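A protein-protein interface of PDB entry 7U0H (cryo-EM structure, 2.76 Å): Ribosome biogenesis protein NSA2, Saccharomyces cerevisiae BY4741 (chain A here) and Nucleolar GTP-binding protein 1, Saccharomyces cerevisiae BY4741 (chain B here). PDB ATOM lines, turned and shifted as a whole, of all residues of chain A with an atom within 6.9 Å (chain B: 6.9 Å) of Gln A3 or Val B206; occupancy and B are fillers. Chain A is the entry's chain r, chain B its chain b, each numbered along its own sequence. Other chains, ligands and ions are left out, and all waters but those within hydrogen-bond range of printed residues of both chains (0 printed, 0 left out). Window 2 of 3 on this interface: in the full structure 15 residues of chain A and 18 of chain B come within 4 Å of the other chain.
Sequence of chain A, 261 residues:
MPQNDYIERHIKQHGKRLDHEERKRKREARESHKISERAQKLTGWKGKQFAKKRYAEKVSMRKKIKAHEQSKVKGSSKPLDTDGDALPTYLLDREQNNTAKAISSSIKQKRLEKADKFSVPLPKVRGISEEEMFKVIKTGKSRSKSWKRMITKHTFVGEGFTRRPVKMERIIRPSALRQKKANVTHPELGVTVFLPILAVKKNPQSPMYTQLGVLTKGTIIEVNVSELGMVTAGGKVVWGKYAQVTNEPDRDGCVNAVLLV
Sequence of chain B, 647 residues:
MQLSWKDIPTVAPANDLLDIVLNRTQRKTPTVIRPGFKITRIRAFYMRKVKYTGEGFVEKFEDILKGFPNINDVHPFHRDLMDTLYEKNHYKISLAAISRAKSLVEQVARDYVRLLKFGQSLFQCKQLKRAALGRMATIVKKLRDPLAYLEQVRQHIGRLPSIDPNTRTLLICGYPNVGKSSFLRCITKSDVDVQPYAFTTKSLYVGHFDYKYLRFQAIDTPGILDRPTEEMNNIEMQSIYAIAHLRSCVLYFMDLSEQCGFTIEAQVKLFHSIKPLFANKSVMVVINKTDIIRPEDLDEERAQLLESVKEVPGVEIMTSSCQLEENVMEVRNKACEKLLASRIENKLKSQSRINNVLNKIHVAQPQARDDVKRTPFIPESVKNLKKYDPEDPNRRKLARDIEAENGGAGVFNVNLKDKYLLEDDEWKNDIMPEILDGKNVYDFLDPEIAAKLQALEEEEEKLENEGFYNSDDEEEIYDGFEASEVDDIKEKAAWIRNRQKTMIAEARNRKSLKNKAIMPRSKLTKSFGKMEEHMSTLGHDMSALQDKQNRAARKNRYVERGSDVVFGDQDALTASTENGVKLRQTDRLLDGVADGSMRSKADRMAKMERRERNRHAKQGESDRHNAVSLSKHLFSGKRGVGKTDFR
Of the 21 printed residues of chain B, 5 touch a printed residue of chain A. Hydrophobic or aromatic side chains of chain B within 4 Å of the printed part of chain A: Pro B161, Tyr B205 and Val B206. Of the 7 printed residues of chain A, 5 touch a printed residue of chain B. Among the printed residues, 11 pairs touch across the chains. Among the printed residues, Asp or Glu carboxylates within 4 Å of a Lys or Arg side-chain nitrogen of the other chain: Asp A5 with Arg B159 (2.6 Å).
Val B206 touches one residue of chain A. Printed residues of chain B within 4 Å of Arg A9: Tyr B205. Printed residues of chain B within 4 Å of Asn A4: Arg B159 (3.0 Å), Pro B161 (3.8 Å), Leu B204 (3.2 Å) and Tyr B205 (3.1 Å). Gln B217 touches none of the printed residues of chain A. Asp B191 touches none of the printed residues of chain A. The nearest printed residue of chain B that does not touch Tyr A6 is Tyr B205 (6.3 Å).
Among the printed residues, merely in contact across the chains: Asn A4 with Tyr B205 (3.1 Å), Gln A3 with Pro B161 (3.4 Å), Gln A3 with Arg B159 (3.7 Å), Tyr A6 with Arg B159 (3.8 Å), Asn A4 with Pro B161 (3.8 Å) and Gln A3 with Tyr B205 (3.9 Å).
O of Val B206 sits at hydrogen-bond distance from OG of Ser B190 (2.7 Å). The backbone carbonyl oxygen (O) of Tyr B205 is in hydrogen-bond range of the backbone NH (N) of Asp B220 (2.9 Å). NH1 of Arg A9 lies within hydrogen-bond range of O of Gln A3, at 2.5 Å.
The backbone NH of Asn A4 is in hydrogen-bond range of the backbone carbonyl oxygen of Arg B159, 3.0 Å away. The guanidinium group of Arg B159 is in salt-bridge range of the side-chain carboxylate of Asp A5, 2.6 Å away. O of Leu B204 is in hydrogen-bond range of ND2 of Asn A4, 3.2 Å away. OH of Tyr B205 is in hydrogen-bond range of NH1 of Arg A9 (3.2 Å). The backbone carbonyl oxygen of Val B206 sits at hydrogen-bond distance from the side-chain amide nitrogen of Gln A3 (3.3 Å).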
ATOM      1  N   PRO A   2      22.346   2.730  27.767  1.00  0.00           N
ATOM      2  CA  PRO A   2      21.971   3.798  26.843  1.00  0.00           C
ATOM      3  C   PRO A   2      21.938   5.146  27.553  1.00  0.00           C
ATOM      4  O   PRO A   2      21.579   5.211  28.728  1.00  0.00           O
ATOM      5  CB  PRO A   2      20.586   3.370  26.388  1.00  0.00           C
ATOM      6  CG  PRO A   2      20.017   2.734  27.600  1.00  0.00           C
ATOM      7  CD  PRO A   2      21.161   2.047  28.304  1.00  0.00           C
ATOM      8  N   GLN A   3      22.323   6.210  26.860  1.00  0.00           N
ATOM      9  CA  GLN A   3      22.403   7.525  27.475  1.00  0.00           C
ATOM     10  C   GLN A   3      21.742   8.566  26.586  1.00  0.00           C
ATOM     11  O   GLN A   3      21.693   8.425  25.361  1.00  0.00           O
ATOM     12  CB  GLN A   3      23.859   7.914  27.757  1.00  0.00           C
ATOM     13  CG  GLN A   3      24.768   7.801  26.557  1.00  0.00           C
ATOM     14  CD  GLN A   3      26.218   7.629  26.944  1.00  0.00           C
ATOM     15  OE1 GLN A   3      26.662   8.136  27.970  1.00  0.00           O
ATOM     16  NE2 GLN A   3      26.962   6.899  26.126  1.00  0.00           N
ATOM     17  N   ASN A   4      21.219   9.603  27.230  1.00  0.00           N
ATOM     18  CA  ASN A   4      20.651  10.790  26.571  1.00  0.00           C
ATOM     19  C   ASN A   4      19.420  10.350  25.774  1.00  0.00           C
ATOM     20  O   ASN A   4      18.674   9.468  26.224  1.00  0.00           O
ATOM     21  CB  ASN A   4      21.725  11.479  25.763  1.00  0.00           C
ATOM     22  CG  ASN A   4      22.967  11.766  26.577  1.00  0.00           C
ATOM     23  OD1 ASN A   4      22.888  12.248  27.703  1.00  0.00           O
ATOM     24  ND2 ASN A   4      24.124  11.453  26.015  1.00  0.00           N
ATOM     25  N   ASP A   5      19.178  10.933  24.605  1.00  0.00           N
ATOM     26  CA  ASP A   5      17.992  10.622  23.813  1.00  0.00           C
ATOM     27  C   ASP A   5      18.235   9.377  22.956  1.00  0.00           C
ATOM     28  O   ASP A   5      18.228   9.415  21.726  1.00  0.00           O
ATOM     29  CB  ASP A   5      17.604  11.823  22.959  1.00  0.00           C
ATOM     30  CG  ASP A   5      17.321  13.059  23.792  1.00  0.00           C
ATOM     31  OD1 ASP A   5      17.523  13.007  25.025  1.00  0.00           O
ATOM     32  OD2 ASP A   5      16.893  14.082  23.218  1.00  0.00           O
ATOM     33  N   TYR A   6      18.429   8.248  23.642  1.00  0.00           N
ATOM     34  CA  TYR A   6      18.840   7.044  22.934  1.00  0.00           C
ATOM     35  C   TYR A   6      17.721   6.454  22.081  1.00  0.00           C
ATOM     36  O   TYR A   6      17.996   5.937  20.997  1.00  0.00           O
ATOM     37  CB  TYR A   6      19.395   6.005  23.909  1.00  0.00           C
ATOM     38  CG  TYR A   6      18.570   5.713  25.140  1.00  0.00           C
ATOM     39  CD1 TYR A   6      17.541   4.786  25.106  1.00  0.00           C
ATOM     40  CD2 TYR A   6      18.867   6.317  26.353  1.00  0.00           C
ATOM     41  CE1 TYR A   6      16.803   4.500  26.234  1.00  0.00           C
ATOM     42  CE2 TYR A   6      18.137   6.036  27.486  1.00  0.00           C
ATOM     43  CZ  TYR A   6      17.106   5.125  27.421  1.00  0.00           C
ATOM     44  OH  TYR A   6      16.376   4.840  28.551  1.00  0.00           O
ATOM     45  N   ILE A   7      16.463   6.530  22.522  1.00  0.00           N
ATOM     46  CA  ILE A   7      15.383   5.973  21.706  1.00  0.00           C
ATOM     47  C   ILE A   7      15.159   6.818  20.458  1.00  0.00           C
ATOM     48  O   ILE A   7      14.930   6.285  19.366  1.00  0.00           O
ATOM     49  CB  ILE A   7      14.094   5.810  22.533  1.00  0.00           C
ATOM     50  CG1 ILE A   7      14.188   4.568  23.415  1.00  0.00           C
ATOM     51  CG2 ILE A   7      12.879   5.691  21.631  1.00  0.00           C
ATOM     52  CD1 ILE A   7      14.414   3.297  22.638  1.00  0.00           C
ATOM     53  N   ARG A   9      17.512   8.596  19.004  1.00  0.00           N
ATOM     54  CA  ARG A   9      18.651   8.260  18.152  1.00  0.00           C
ATOM     55  C   ARG A   9      18.433   6.929  17.448  1.00  0.00           C
ATOM     56  O   ARG A   9      18.810   6.765  16.284  1.00  0.00           O
ATOM     57  CB  ARG A   9      19.945   8.221  18.967  1.00  0.00           C
ATOM     58  CG  ARG A   9      20.392   9.562  19.531  1.00  0.00           C
ATOM     59  CD  ARG A   9      21.808   9.494  20.087  1.00  0.00           C
ATOM     60  NE  ARG A   9      22.130   8.183  20.640  1.00  0.00           N
ATOM     61  CZ  ARG A   9      22.130   7.882  21.931  1.00  0.00           C
ATOM     62  NH1 ARG A   9      21.829   8.782  22.852  1.00  0.00           N
ATOM     63  NH2 ARG A   9      22.436   6.645  22.307  1.00  0.00           N
ATOM     64  N   ARG B 159      17.460   9.346  32.142  1.00  0.00           N
ATOM     65  CA  ARG B 159      18.216   9.116  30.917  1.00  0.00           C
ATOM     66  C   ARG B 159      19.658   9.612  30.980  1.00  0.00           C
ATOM     67  O   ARG B 159      20.441   9.274  30.088  1.00  0.00           O
ATOM     68  CB  ARG B 159      17.512   9.765  29.727  1.00  0.00           C
ATOM     69  CG  ARG B 159      16.356   8.953  29.186  1.00  0.00           C
ATOM     70  CD  ARG B 159      15.821   9.580  27.921  1.00  0.00           C
ATOM     71  NE  ARG B 159      15.403  10.955  28.157  1.00  0.00           N
ATOM     72  CZ  ARG B 159      15.274  11.870  27.209  1.00  0.00           C
ATOM     73  NH1 ARG B 159      15.525  11.591  25.942  1.00  0.00           N
ATOM     74  NH2 ARG B 159      14.897  13.098  27.541  1.00  0.00           N
ATOM     75  N   LEU B 160      20.029  10.399  31.990  1.00  0.00           N
ATOM     76  CA  LEU B 160      21.410  10.861  32.096  1.00  0.00           C
ATOM     77  C   LEU B 160      22.374   9.689  32.301  1.00  0.00           C
ATOM     78  O   LEU B 160      21.996   8.651  32.852  1.00  0.00           O
ATOM     79  CB  LEU B 160      21.564  11.845  33.251  1.00  0.00           C
ATOM     80  CG  LEU B 160      21.111  13.282  33.009  1.00  0.00           C
ATOM     81  CD1 LEU B 160      21.345  14.104  34.257  1.00  0.00           C
ATOM     82  CD2 LEU B 160      21.839  13.876  31.823  1.00  0.00           C
ATOM     83  N   PRO B 161      23.642   9.834  31.867  1.00  0.00           N
ATOM     84  CA  PRO B 161      24.619   8.751  32.056  1.00  0.00           C
ATOM     85  C   PRO B 161      25.117   8.622  33.486  1.00  0.00           C
ATOM     86  O   PRO B 161      24.625   9.298  34.393  1.00  0.00           O
ATOM     87  CB  PRO B 161      25.759   9.139  31.107  1.00  0.00           C
ATOM     88  CG  PRO B 161      25.649  10.607  30.975  1.00  0.00           C
ATOM     89  CD  PRO B 161      24.189  10.933  31.054  1.00  0.00           C
ATOM     90  N   SER B 162      26.094   7.743  33.693  1.00  0.00           N
ATOM     91  CA  SER B 162      26.643   7.438  35.012  1.00  0.00           C
ATOM     92  C   SER B 162      28.138   7.741  34.986  1.00  0.00           C
ATOM     93  O   SER B 162      28.954   6.871  34.674  1.00  0.00           O
ATOM     94  CB  SER B 162      26.372   5.975  35.385  1.00  0.00           C
ATOM     95  OG  SER B 162      26.574   5.742  36.766  1.00  0.00           O
ATOM     96  N   ILE B 163      28.497   8.976  35.319  1.00  0.00           N
ATOM     97  CA  ILE B 163      29.889   9.408  35.382  1.00  0.00           C
ATOM     98  C   ILE B 163      30.284   9.495  36.847  1.00  0.00           C
ATOM     99  O   ILE B 163      29.683  10.255  37.615  1.00  0.00           O
ATOM    100  CB  ILE B 163      30.101  10.753  34.672  1.00  0.00           C
ATOM    101  CG1 ILE B 163      30.097  10.563  33.158  1.00  0.00           C
ATOM    102  CG2 ILE B 163      31.400  11.401  35.129  1.00  0.00           C
ATOM    103  CD1 ILE B 163      30.038  11.860  32.381  1.00  0.00           C
ATOM    104  N   ASP B 164      31.292   8.717  37.236  1.00  0.00           N
ATOM    105  CA  ASP B 164      31.831   8.788  38.588  1.00  0.00           C
ATOM    106  C   ASP B 164      33.011   9.748  38.615  1.00  0.00           C
ATOM    107  O   ASP B 164      34.017   9.491  37.943  1.00  0.00           O
ATOM    108  CB  ASP B 164      32.266   7.418  39.071  1.00  0.00           C
ATOM    109  CG  ASP B 164      33.096   7.483  40.336  1.00  0.00           C
ATOM    110  OD1 ASP B 164      32.691   8.185  41.283  1.00  0.00           O
ATOM    111  OD2 ASP B 164      34.152   6.824  40.386  1.00  0.00           O
ATOM    112  N   LEU B 184      36.293   8.973  20.211  1.00  0.00           N
ATOM    113  CA  LEU B 184      35.577   8.217  21.228  1.00  0.00           C
ATOM    114  C   LEU B 184      35.089   6.887  20.680  1.00  0.00           C
ATOM    115  O   LEU B 184      35.244   5.851  21.333  1.00  0.00           O
ATOM    116  CB  LEU B 184      34.407   9.025  21.781  1.00  0.00           C
ATOM    117  CG  LEU B 184      33.788   8.355  23.009  1.00  0.00           C
ATOM    118  CD1 LEU B 184      34.853   8.168  24.076  1.00  0.00           C
ATOM    119  CD2 LEU B 184      32.614   9.149  23.552  1.00  0.00           C
ATOM    120  N   THR B 188      36.653   3.577  22.385  1.00  0.00           N
ATOM    121  CA  THR B 188      35.587   2.920  23.125  1.00  0.00           C
ATOM    122  C   THR B 188      34.455   2.602  22.161  1.00  0.00           C
ATOM    123  O   THR B 188      34.399   3.122  21.046  1.00  0.00           O
ATOM    124  CB  THR B 188      35.055   3.794  24.271  1.00  0.00           C
ATOM    125  OG1 THR B 188      34.392   4.938  23.724  1.00  0.00           O
ATOM    126  CG2 THR B 188      36.178   4.255  25.178  1.00  0.00           C
ATOM    127  N   LYS B 189      33.540   1.741  22.601  1.00  0.00           N
ATOM    128  CA  LYS B 189      32.349   1.419  21.814  1.00  0.00           C
ATOM    129  C   LYS B 189      31.171   2.307  22.232  1.00  0.00           C
ATOM    130  O   LYS B 189      30.105   1.841  22.631  1.00  0.00           O
ATOM    131  CB  LYS B 189      32.009  -0.062  21.947  1.00  0.00           C
ATOM    132  CG  LYS B 189      31.970  -0.586  23.373  1.00  0.00           C
ATOM    133  CD  LYS B 189      31.589  -2.051  23.402  1.00  0.00           C
ATOM    134  CE  LYS B 189      32.525  -2.870  22.533  1.00  0.00           C
ATOM    135  NZ  LYS B 189      32.176  -4.315  22.554  1.00  0.00           N
ATOM    136  N   SER B 190      31.383   3.617  22.120  1.00  0.00           N
ATOM    137  CA  SER B 190      30.339   4.599  22.383  1.00  0.00           C
ATOM    138  C   SER B 190      29.662   5.000  21.080  1.00  0.00           C
ATOM    139  O   SER B 190      30.317   5.149  20.044  1.00  0.00           O
ATOM    140  CB  SER B 190      30.912   5.833  23.081  1.00  0.00           C
ATOM    141  OG  SER B 190      31.329   5.519  24.396  1.00  0.00           O
ATOM    142  N   ASP B 191      28.348   5.201  21.150  1.00  0.00           N
ATOM    143  CA  ASP B 191      27.470   5.286  19.982  1.00  0.00           C
ATOM    144  C   ASP B 191      27.123   6.725  19.609  1.00  0.00           C
ATOM    145  O   ASP B 191      25.992   7.006  19.207  1.00  0.00           O
ATOM    146  CB  ASP B 191      26.199   4.476  20.238  1.00  0.00           C
ATOM    147  CG  ASP B 191      25.436   4.150  18.961  1.00  0.00           C
ATOM    148  OD1 ASP B 191      25.981   4.369  17.860  1.00  0.00           O
ATOM    149  OD2 ASP B 191      24.286   3.674  19.064  1.00  0.00           O
ATOM    150  N   VAL B 192      28.064   7.665  19.733  1.00  0.00           N
ATOM    151  CA  VAL B 192      27.759   9.048  19.367  1.00  0.00           C
ATOM    152  C   VAL B 192      27.673   9.181  17.846  1.00  0.00           C
ATOM    153  O   VAL B 192      28.118   8.313  17.083  1.00  0.00           O
ATOM    154  CB  VAL B 192      28.800  10.015  19.956  1.00  0.00           C
ATOM    155  CG1 VAL B 192      30.032  10.082  19.071  1.00  0.00           C
ATOM    156  CG2 VAL B 192      28.198  11.402  20.168  1.00  0.00           C
ATOM    157  N   LEU B 204      26.824  15.571  27.258  1.00  0.00           N
ATOM    158  CA  LEU B 204      28.038  14.805  27.500  1.00  0.00           C
ATOM    159  C   LEU B 204      27.838  13.351  27.096  1.00  0.00           C
ATOM    160  O   LEU B 204      26.742  12.798  27.224  1.00  0.00           O
ATOM    161  CB  LEU B 204      28.430  14.869  28.975  1.00  0.00           C
ATOM    162  CG  LEU B 204      28.204  16.181  29.723  1.00  0.00           C
ATOM    163  CD1 LEU B 204      28.600  16.040  31.185  1.00  0.00           C
ATOM    164  CD2 LEU B 204      28.978  17.301  29.070  1.00  0.00           C
ATOM    165  N   TYR B 205      28.907  12.720  26.614  1.00  0.00           N
ATOM    166  CA  TYR B 205      28.848  11.303  26.287  1.00  0.00           C
ATOM    167  C   TYR B 205      29.974  10.557  26.982  1.00  0.00           C
ATOM    168  O   TYR B 205      31.052  11.105  27.211  1.00  0.00           O
ATOM    169  CB  TYR B 205      28.904  11.073  24.778  1.00  0.00           C
ATOM    170  CG  TYR B 205      27.539  11.139  24.144  1.00  0.00           C
ATOM    171  CD1 TYR B 205      26.884  12.354  23.985  1.00  0.00           C
ATOM    172  CD2 TYR B 205      26.892   9.986  23.726  1.00  0.00           C
ATOM    173  CE1 TYR B 205      25.630  12.422  23.414  1.00  0.00           C
ATOM    174  CE2 TYR B 205      25.634  10.043  23.151  1.00  0.00           C
ATOM    175  CZ  TYR B 205      25.008  11.262  22.998  1.00  0.00           C
ATOM    176  OH  TYR B 205      23.754  11.328  22.427  1.00  0.00           O
ATOM    177  N   VAL B 206      29.714   9.302  27.328  1.00  0.00           N
ATOM    178  CA  VAL B 206      30.647   8.518  28.126  1.00  0.00           C
ATOM    179  C   VAL B 206      30.976   7.225  27.397  1.00  0.00           C
ATOM    180  O   VAL B 206      30.202   6.726  26.576  1.00  0.00           O
ATOM    181  CB  VAL B 206      30.092   8.212  29.533  1.00  0.00           C
ATOM    182  CG1 VAL B 206      31.226   8.072  30.534  1.00  0.00           C
ATOM    183  CG2 VAL B 206      29.127   9.286  29.966  1.00  0.00           C
ATOM    184  N   GLY B 207      32.153   6.692  27.709  1.00  0.00           N
ATOM    185  CA  GLY B 207      32.589   5.397  27.227  1.00  0.00           C
ATOM    186  C   GLY B 207      33.606   4.849  28.199  1.00  0.00           C
ATOM    187  O   GLY B 207      34.063   5.546  29.104  1.00  0.00           O
ATOM    188  N   HIS B 208      33.971   3.588  28.002  1.00  0.00           N
ATOM    189  CA  HIS B 208      34.893   2.937  28.917  1.00  0.00           C
ATOM    190  C   HIS B 208      35.921   2.133  28.138  1.00  0.00           C
ATOM    191  O   HIS B 208      35.662   1.682  27.020  1.00  0.00           O
ATOM    192  CB  HIS B 208      34.150   2.028  29.903  1.00  0.00           C
ATOM    193  CG  HIS B 208      33.179   2.758  30.777  1.00  0.00           C
ATOM    194  ND1 HIS B 208      33.452   3.074  32.090  1.00  0.00           N
ATOM    195  CD2 HIS B 208      31.940   3.239  30.526  1.00  0.00           C
ATOM    196  CE1 HIS B 208      32.423   3.715  32.610  1.00  0.00           C
ATOM    197  NE2 HIS B 208      31.492   3.828  31.682  1.00  0.00           N
ATOM    198  N   GLN B 217      37.598   5.528  32.155  1.00  0.00           N
ATOM    199  CA  GLN B 217      36.458   6.032  31.412  1.00  0.00           C
ATOM    200  C   GLN B 217      36.889   7.225  30.571  1.00  0.00           C
ATOM    201  O   GLN B 217      37.906   7.864  30.838  1.00  0.00           O
ATOM    202  CB  GLN B 217      35.308   6.422  32.345  1.00  0.00           C
ATOM    203  CG  GLN B 217      35.643   7.489  33.352  1.00  0.00           C
ATOM    204  CD  GLN B 217      34.492   7.759  34.292  1.00  0.00           C
ATOM    205  OE1 GLN B 217      34.682   8.249  35.404  1.00  0.00           O
ATOM    206  NE2 GLN B 217      33.286   7.442  33.849  1.00  0.00           N
ATOM    207  N   ALA B 218      36.108   7.505  29.535  1.00  0.00           N
ATOM    208  CA  ALA B 218      36.393   8.585  28.605  1.00  0.00           C
ATOM    209  C   ALA B 218      35.128   9.399  28.396  1.00  0.00           C
ATOM    210  O   ALA B 218      34.064   8.837  28.119  1.00  0.00           O
ATOM    211  CB  ALA B 218      36.907   8.045  27.269  1.00  0.00           C
ATOM    212  N   ILE B 219      35.244  10.716  28.517  1.00  0.00           N
ATOM    213  CA  ILE B 219      34.108  11.619  28.376  1.00  0.00           C
ATOM    214  C   ILE B 219      34.335  12.485  27.150  1.00  0.00           C
ATOM    215  O   ILE B 219      35.444  12.985  26.938  1.00  0.00           O
ATOM    216  CB  ILE B 219      33.900  12.487  29.631  1.00  0.00           C
ATOM    217  CG1 ILE B 219      33.480  11.621  30.816  1.00  0.00           C
ATOM    218  CG2 ILE B 219      32.848  13.559  29.379  1.00  0.00           C
ATOM    219  CD1 ILE B 219      34.623  11.109  31.637  1.00  0.00           C
ATOM    220  N   ASP B 220      33.297  12.634  26.334  1.00  0.00           N
ATOM    221  CA  ASP B 220      33.312  13.483  25.151  1.00  0.00           C
ATOM    222  C   ASP B 220      32.361  14.651  25.374  1.00  0.00           C
ATOM    223  O   ASP B 220      31.198  14.447  25.752  1.00  0.00           O
ATOM    224  CB  ASP B 220      32.901  12.690  23.911  1.00  0.00           C
ATOM    225  CG  ASP B 220      33.281  13.379  22.619  1.00  0.00           C
ATOM    226  OD1 ASP B 220      33.317  14.627  22.587  1.00  0.00           O
ATOM    227  OD2 ASP B 220      33.543  12.668  21.629  1.00  0.00           O
